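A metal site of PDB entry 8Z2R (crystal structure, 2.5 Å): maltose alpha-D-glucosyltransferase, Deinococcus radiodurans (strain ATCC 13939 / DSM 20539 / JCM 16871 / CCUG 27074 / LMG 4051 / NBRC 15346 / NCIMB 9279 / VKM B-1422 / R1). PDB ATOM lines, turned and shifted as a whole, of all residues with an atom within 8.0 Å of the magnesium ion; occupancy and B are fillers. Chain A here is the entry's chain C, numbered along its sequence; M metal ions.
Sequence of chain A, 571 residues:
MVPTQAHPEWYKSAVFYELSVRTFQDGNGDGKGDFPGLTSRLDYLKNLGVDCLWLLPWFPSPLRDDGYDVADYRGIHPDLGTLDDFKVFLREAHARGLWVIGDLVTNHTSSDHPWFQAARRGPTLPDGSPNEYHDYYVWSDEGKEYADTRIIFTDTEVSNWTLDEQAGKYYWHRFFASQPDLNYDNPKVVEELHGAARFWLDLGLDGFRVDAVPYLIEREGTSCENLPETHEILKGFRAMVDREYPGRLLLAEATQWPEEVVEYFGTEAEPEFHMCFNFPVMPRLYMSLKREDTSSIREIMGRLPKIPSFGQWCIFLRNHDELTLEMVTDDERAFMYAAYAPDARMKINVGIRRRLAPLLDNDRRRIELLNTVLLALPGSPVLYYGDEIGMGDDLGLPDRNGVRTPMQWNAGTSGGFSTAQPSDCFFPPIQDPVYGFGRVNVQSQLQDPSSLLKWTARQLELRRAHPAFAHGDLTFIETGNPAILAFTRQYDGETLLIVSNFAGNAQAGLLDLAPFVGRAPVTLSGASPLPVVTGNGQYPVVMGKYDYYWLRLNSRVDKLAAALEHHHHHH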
ATOM      1  N   VAL A  21      12.517  -6.029 -24.650  1.00  0.00           N
ATOM      2  CA  VAL A  21      13.798  -6.728 -24.683  1.00  0.00           C
ATOM      3  C   VAL A  21      13.594  -8.224 -24.902  1.00  0.00           C
ATOM      4  O   VAL A  21      14.371  -8.869 -25.614  1.00  0.00           O
ATOM      5  CB  VAL A  21      14.562  -6.436 -23.382  1.00  0.00           C
ATOM      6  CG1 VAL A  21      16.039  -6.830 -23.521  1.00  0.00           C
ATOM      7  CG2 VAL A  21      14.355  -4.957 -22.972  1.00  0.00           C
ATOM      8  N   ARG A  22      12.534  -8.789 -24.306  1.00  0.00           N
ATOM      9  CA  ARG A  22      12.282 -10.233 -24.375  1.00  0.00           C
ATOM     10  C   ARG A  22      12.061 -10.697 -25.807  1.00  0.00           C
ATOM     11  O   ARG A  22      12.439 -11.817 -26.176  1.00  0.00           O
ATOM     12  CB  ARG A  22      11.049 -10.586 -23.543  1.00  0.00           C
ATOM     13  CG  ARG A  22      10.850 -12.091 -23.329  1.00  0.00           C
ATOM     14  CD  ARG A  22      10.125 -12.354 -22.030  1.00  0.00           C
ATOM     15  NE  ARG A  22      10.908 -11.901 -20.888  1.00  0.00           N
ATOM     16  CZ  ARG A  22      10.584 -10.864 -20.135  1.00  0.00           C
ATOM     17  NH1 ARG A  22       9.484 -10.161 -20.369  1.00  0.00           N
ATOM     18  NH2 ARG A  22      11.394 -10.513 -19.141  1.00  0.00           N
ATOM     19  N   GLN A  25      15.785  -9.405 -29.370  1.00  0.00           N
ATOM     20  CA  GLN A  25      16.904 -10.187 -29.892  1.00  0.00           C
ATOM     21  C   GLN A  25      17.486 -11.063 -28.800  1.00  0.00           C
ATOM     22  O   GLN A  25      17.944 -10.560 -27.767  1.00  0.00           O
ATOM     23  CB  GLN A  25      17.964  -9.290 -30.497  1.00  0.00           C
ATOM     24  CG  GLN A  25      19.215 -10.007 -30.941  1.00  0.00           C
ATOM     25  CD  GLN A  25      19.001 -10.842 -32.197  1.00  0.00           C
ATOM     26  OE1 GLN A  25      19.182 -10.361 -33.314  1.00  0.00           O
ATOM     27  NE2 GLN A  25      18.592 -12.089 -32.007  1.00  0.00           N
ATOM     28  N   ASP A  26      17.478 -12.375 -29.041  1.00  0.00           N
ATOM     29  CA  ASP A  26      18.073 -13.339 -28.121  1.00  0.00           C
ATOM     30  C   ASP A  26      19.574 -13.404 -28.372  1.00  0.00           C
ATOM     31  O   ASP A  26      20.003 -13.633 -29.501  1.00  0.00           O
ATOM     32  CB  ASP A  26      17.425 -14.717 -28.321  1.00  0.00           C
ATOM     33  CG  ASP A  26      18.256 -15.870 -27.768  1.00  0.00           C
ATOM     34  OD1 ASP A  26      18.735 -15.760 -26.622  1.00  0.00           O
ATOM     35  OD2 ASP A  26      18.412 -16.892 -28.469  1.00  0.00           O
ATOM     36  N   GLY A  27      20.365 -13.209 -27.334  1.00  0.00           N
ATOM     37  CA  GLY A  27      21.788 -13.308 -27.515  1.00  0.00           C
ATOM     38  C   GLY A  27      22.395 -14.649 -27.177  1.00  0.00           C
ATOM     39  O   GLY A  27      23.427 -15.003 -27.752  1.00  0.00           O
ATOM     40  N   ASN A  28      21.776 -15.399 -26.255  1.00  0.00           N
ATOM     41  CA  ASN A  28      22.384 -16.610 -25.698  1.00  0.00           C
ATOM     42  C   ASN A  28      21.952 -17.903 -26.372  1.00  0.00           C
ATOM     43  O   ASN A  28      22.769 -18.820 -26.495  1.00  0.00           O
ATOM     44  CB  ASN A  28      22.105 -16.717 -24.183  1.00  0.00           C
ATOM     45  CG  ASN A  28      20.672 -16.369 -23.812  1.00  0.00           C
ATOM     46  OD1 ASN A  28      20.041 -15.535 -24.460  1.00  0.00           O
ATOM     47  ND2 ASN A  28      20.160 -16.966 -22.744  1.00  0.00           N
ATOM     48  N   GLY A  29      20.676 -18.026 -26.764  1.00  0.00           N
ATOM     49  CA  GLY A  29      20.214 -19.245 -27.421  1.00  0.00           C
ATOM     50  C   GLY A  29      18.959 -19.870 -26.843  1.00  0.00           C
ATOM     51  O   GLY A  29      18.491 -20.903 -27.339  1.00  0.00           O
ATOM     52  N   ASP A  30      18.379 -19.265 -25.825  1.00  0.00           N
ATOM     53  CA  ASP A  30      17.243 -19.826 -25.099  1.00  0.00           C
ATOM     54  C   ASP A  30      15.906 -19.288 -25.593  1.00  0.00           C
ATOM     55  O   ASP A  30      14.889 -19.449 -24.901  1.00  0.00           O
ATOM     56  CB  ASP A  30      17.370 -19.531 -23.617  1.00  0.00           C
ATOM     57  CG  ASP A  30      17.231 -18.050 -23.316  1.00  0.00           C
ATOM     58  OD1 ASP A  30      17.932 -17.259 -23.968  1.00  0.00           O
ATOM     59  OD2 ASP A  30      16.399 -17.683 -22.469  1.00  0.00           O
ATOM     60  N   GLY A  31      15.868 -18.635 -26.751  1.00  0.00           N
ATOM     61  CA  GLY A  31      14.617 -18.143 -27.265  1.00  0.00           C
ATOM     62  C   GLY A  31      14.032 -16.984 -26.505  1.00  0.00           C
ATOM     63  O   GLY A  31      12.817 -16.738 -26.582  1.00  0.00           O
ATOM     64  N   LYS A  32      14.869 -16.251 -25.766  1.00  0.00           N
ATOM     65  CA  LYS A  32      14.390 -15.087 -25.027  1.00  0.00           C
ATOM     66  C   LYS A  32      15.338 -13.929 -25.261  1.00  0.00           C
ATOM     67  O   LYS A  32      16.542 -14.046 -25.018  1.00  0.00           O
ATOM     68  CB  LYS A  32      14.265 -15.412 -23.535  1.00  0.00           C
ATOM     69  CG  LYS A  32      13.443 -16.667 -23.227  1.00  0.00           C
ATOM     70  CD  LYS A  32      12.845 -16.613 -21.847  1.00  0.00           C
ATOM     71  CE  LYS A  32      12.502 -17.986 -21.284  1.00  0.00           C
ATOM     72  NZ  LYS A  32      11.794 -17.837 -19.997  1.00  0.00           N
ATOM     73  N   GLY A  33      14.805 -12.818 -25.761  1.00  0.00           N
ATOM     74  CA  GLY A  33      15.641 -11.676 -26.076  1.00  0.00           C
ATOM     75  C   GLY A  33      16.267 -11.101 -24.820  1.00  0.00           C
ATOM     76  O   GLY A  33      15.542 -10.736 -23.878  1.00  0.00           O
ATOM     77  N   ASP A  34      17.603 -11.011 -24.791  1.00  0.00           N
ATOM     78  CA  ASP A  34      18.336 -10.510 -23.637  1.00  0.00           C
ATOM     79  C   ASP A  34      19.049  -9.199 -23.952  1.00  0.00           C
ATOM     80  O   ASP A  34      19.251  -8.847 -25.117  1.00  0.00           O
ATOM     81  CB  ASP A  34      19.340 -11.567 -23.162  1.00  0.00           C
ATOM     82  CG  ASP A  34      20.370 -11.899 -24.214  1.00  0.00           C
ATOM     83  OD1 ASP A  34      20.818 -11.005 -24.958  1.00  0.00           O
ATOM     84  OD2 ASP A  34      20.784 -13.072 -24.302  1.00  0.00           O
ATOM     85  N   PHE A  35      19.460  -8.487 -22.888  1.00  0.00           N
ATOM     86  CA  PHE A  35      20.154  -7.214 -23.071  1.00  0.00           C
ATOM     87  C   PHE A  35      21.413  -7.342 -23.921  1.00  0.00           C
ATOM     88  O   PHE A  35      21.586  -6.514 -24.831  1.00  0.00           O
ATOM     89  CB  PHE A  35      20.469  -6.543 -21.725  1.00  0.00           C
ATOM     90  CG  PHE A  35      19.366  -5.644 -21.241  1.00  0.00           C
ATOM     91  CD1 PHE A  35      19.258  -4.348 -21.709  1.00  0.00           C
ATOM     92  CD2 PHE A  35      18.399  -6.123 -20.378  1.00  0.00           C
ATOM     93  CE1 PHE A  35      18.200  -3.529 -21.290  1.00  0.00           C
ATOM     94  CE2 PHE A  35      17.361  -5.318 -19.962  1.00  0.00           C
ATOM     95  CZ  PHE A  35      17.267  -4.013 -20.413  1.00  0.00           C
ATOM     96  N   PRO A  36      22.299  -8.324 -23.729  1.00  0.00           N
ATOM     97  CA  PRO A  36      23.454  -8.446 -24.643  1.00  0.00           C
ATOM     98  C   PRO A  36      23.062  -8.506 -26.102  1.00  0.00           C
ATOM     99  O   PRO A  36      23.837  -8.054 -26.969  1.00  0.00           O
ATOM    100  CB  PRO A  36      24.119  -9.758 -24.213  1.00  0.00           C
ATOM    101  CG  PRO A  36      23.729  -9.931 -22.823  1.00  0.00           C
ATOM    102  CD  PRO A  36      22.362  -9.286 -22.628  1.00  0.00           C
ATOM    103  N   GLY A  37      21.898  -9.081 -26.400  1.00  0.00           N
ATOM    104  CA  GLY A  37      21.460  -9.174 -27.783  1.00  0.00           C
ATOM    105  C   GLY A  37      20.921  -7.863 -28.310  1.00  0.00           C
ATOM    106  O   GLY A  37      21.261  -7.444 -29.425  1.00  0.00           O
ATOM    107  N   PRO A  78      15.607 -12.061 -14.946  1.00  0.00           N
ATOM    108  CA  PRO A  78      16.703 -12.943 -15.387  1.00  0.00           C
ATOM    109  C   PRO A  78      16.551 -13.435 -16.806  1.00  0.00           C
ATOM    110  O   PRO A  78      17.505 -14.025 -17.351  1.00  0.00           O
ATOM    111  CB  PRO A  78      16.636 -14.116 -14.397  1.00  0.00           C
ATOM    112  CG  PRO A  78      15.852 -13.595 -13.241  1.00  0.00           C
ATOM    113  CD  PRO A  78      14.867 -12.624 -13.807  1.00  0.00           C
ATOM    114  N   ASP A  79      15.395 -13.238 -17.420  1.00  0.00           N
ATOM    115  CA  ASP A  79      15.205 -13.650 -18.802  1.00  0.00           C
ATOM    116  C   ASP A  79      16.100 -12.815 -19.716  1.00  0.00           C
ATOM    117  O   ASP A  79      16.784 -13.341 -20.611  1.00  0.00           O
ATOM    118  CB  ASP A  79      13.745 -13.475 -19.176  1.00  0.00           C
ATOM    119  CG  ASP A  79      12.943 -14.687 -18.848  1.00  0.00           C
ATOM    120  OD1 ASP A  79      13.519 -15.803 -18.859  1.00  0.00           O
ATOM    121  OD2 ASP A  79      11.720 -14.530 -18.611  1.00  0.00           O
ATOM    122  N   LEU A  80      16.135 -11.503 -19.440  1.00  0.00           N
ATOM    123  CA  LEU A  80      16.788 -10.433 -20.176  1.00  0.00           C
ATOM    124  C   LEU A  80      18.263 -10.300 -19.823  1.00  0.00           C
ATOM    125  O   LEU A  80      18.937  -9.428 -20.384  1.00  0.00           O
ATOM    126  CB  LEU A  80      16.074  -9.130 -19.866  1.00  0.00           C
ATOM    127  CG  LEU A  80      14.580  -9.402 -19.785  1.00  0.00           C
ATOM    128  CD1 LEU A  80      13.825  -8.210 -19.226  1.00  0.00           C
ATOM    129  CD2 LEU A  80      14.043  -9.808 -21.172  1.00  0.00           C
ATOM    130  N   GLY A  81      18.758 -11.133 -18.914  1.00  0.00           N
ATOM    131  CA  GLY A  81      20.144 -11.038 -18.478  1.00  0.00           C
ATOM    132  C   GLY A  81      20.285 -10.223 -17.208  1.00  0.00           C
ATOM    133  O   GLY A  81      19.330  -9.951 -16.467  1.00  0.00           O
ATOM    134  N   PHE A 417      16.011 -14.042 -34.935  1.00  0.00           N
ATOM    135  CA  PHE A 417      15.744 -13.577 -33.588  1.00  0.00           C
ATOM    136  C   PHE A 417      16.409 -14.462 -32.537  1.00  0.00           C
ATOM    137  O   PHE A 417      16.718 -13.982 -31.447  1.00  0.00           O
ATOM    138  CB  PHE A 417      14.249 -13.548 -33.329  1.00  0.00           C
ATOM    139  CG  PHE A 417      13.902 -13.647 -31.886  1.00  0.00           C
ATOM    140  CD1 PHE A 417      13.979 -12.535 -31.042  1.00  0.00           C
ATOM    141  CD2 PHE A 417      13.591 -14.885 -31.321  1.00  0.00           C
ATOM    142  CE1 PHE A 417      13.688 -12.639 -29.696  1.00  0.00           C
ATOM    143  CE2 PHE A 417      13.301 -14.988 -29.975  1.00  0.00           C
ATOM    144  CZ  PHE A 417      13.340 -13.858 -29.160  1.00  0.00           C
ATOM    145  N   SER A 418      16.626 -15.744 -32.832  1.00  0.00           N
ATOM    146  CA  SER A 418      17.267 -16.678 -31.924  1.00  0.00           C
ATOM    147  C   SER A 418      17.765 -17.883 -32.703  1.00  0.00           C
ATOM    148  O   SER A 418      17.297 -18.166 -33.799  1.00  0.00           O
ATOM    149  CB  SER A 418      16.330 -17.177 -30.832  1.00  0.00           C
ATOM    150  OG  SER A 418      16.781 -18.437 -30.387  1.00  0.00           O
HETATM  151 MG    MG M   1      18.225 -15.004 -24.525  1.00  0.00          MG
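N of Gly 27 touches the magnesium ion, 3.96 Å away. OD2 of Asp 34 touches the magnesium ion, at 3.2 Å. Along chain A the residues within 4 Å of the magnesium ion span positions 26 to 34.
OD2 of Asp 34 sits at hydrogen-bond distance from N of Asn 28 (3.2 Å). The side-chain carboxylate (OD1) of Asp 79 is in salt-bridge range of the side-chain amino group (NZ) of Lys 32 (2.9 Å). N of Gly 29 is in hydrogen-bond range of OD2 of Asp 26 (3.1 Å). The backbone NH (N) of Asp 26 is in hydrogen-bond range of the backbone carbonyl oxygen (O) of Phe 417, at 3.0 Å. The side-chain hydroxyl of Ser 418 is in hydrogen-bond range of the side-chain carboxylate of Asp 26 (3.0 Å). The side-chain carboxylate (OD2) of Asp 34 lies within hydrogen-bond range of the backbone NH (N) of Gly 27, 3.1 Å away. N of Asp 34 is in hydrogen-bond range of O of Gln 25 (3.0 Å). The side-chain carboxylate (OD1) of Asp 34 is in hydrogen-bond range of the backbone NH (N) of Gly 37 (2.6 Å).
OD1 of Asn 28 is bound to the magnesium ion, at 1.9 Å. O of Lys 32 binds the magnesium ion, 2.0 Å away. OD1 of Asp 26 is bound to the magnesium ion (2.3 Å). The magnesium ion is bound by OD1 of Asp 30 (2.3 Å). The magnesium ion has four donor atoms within binding distance.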
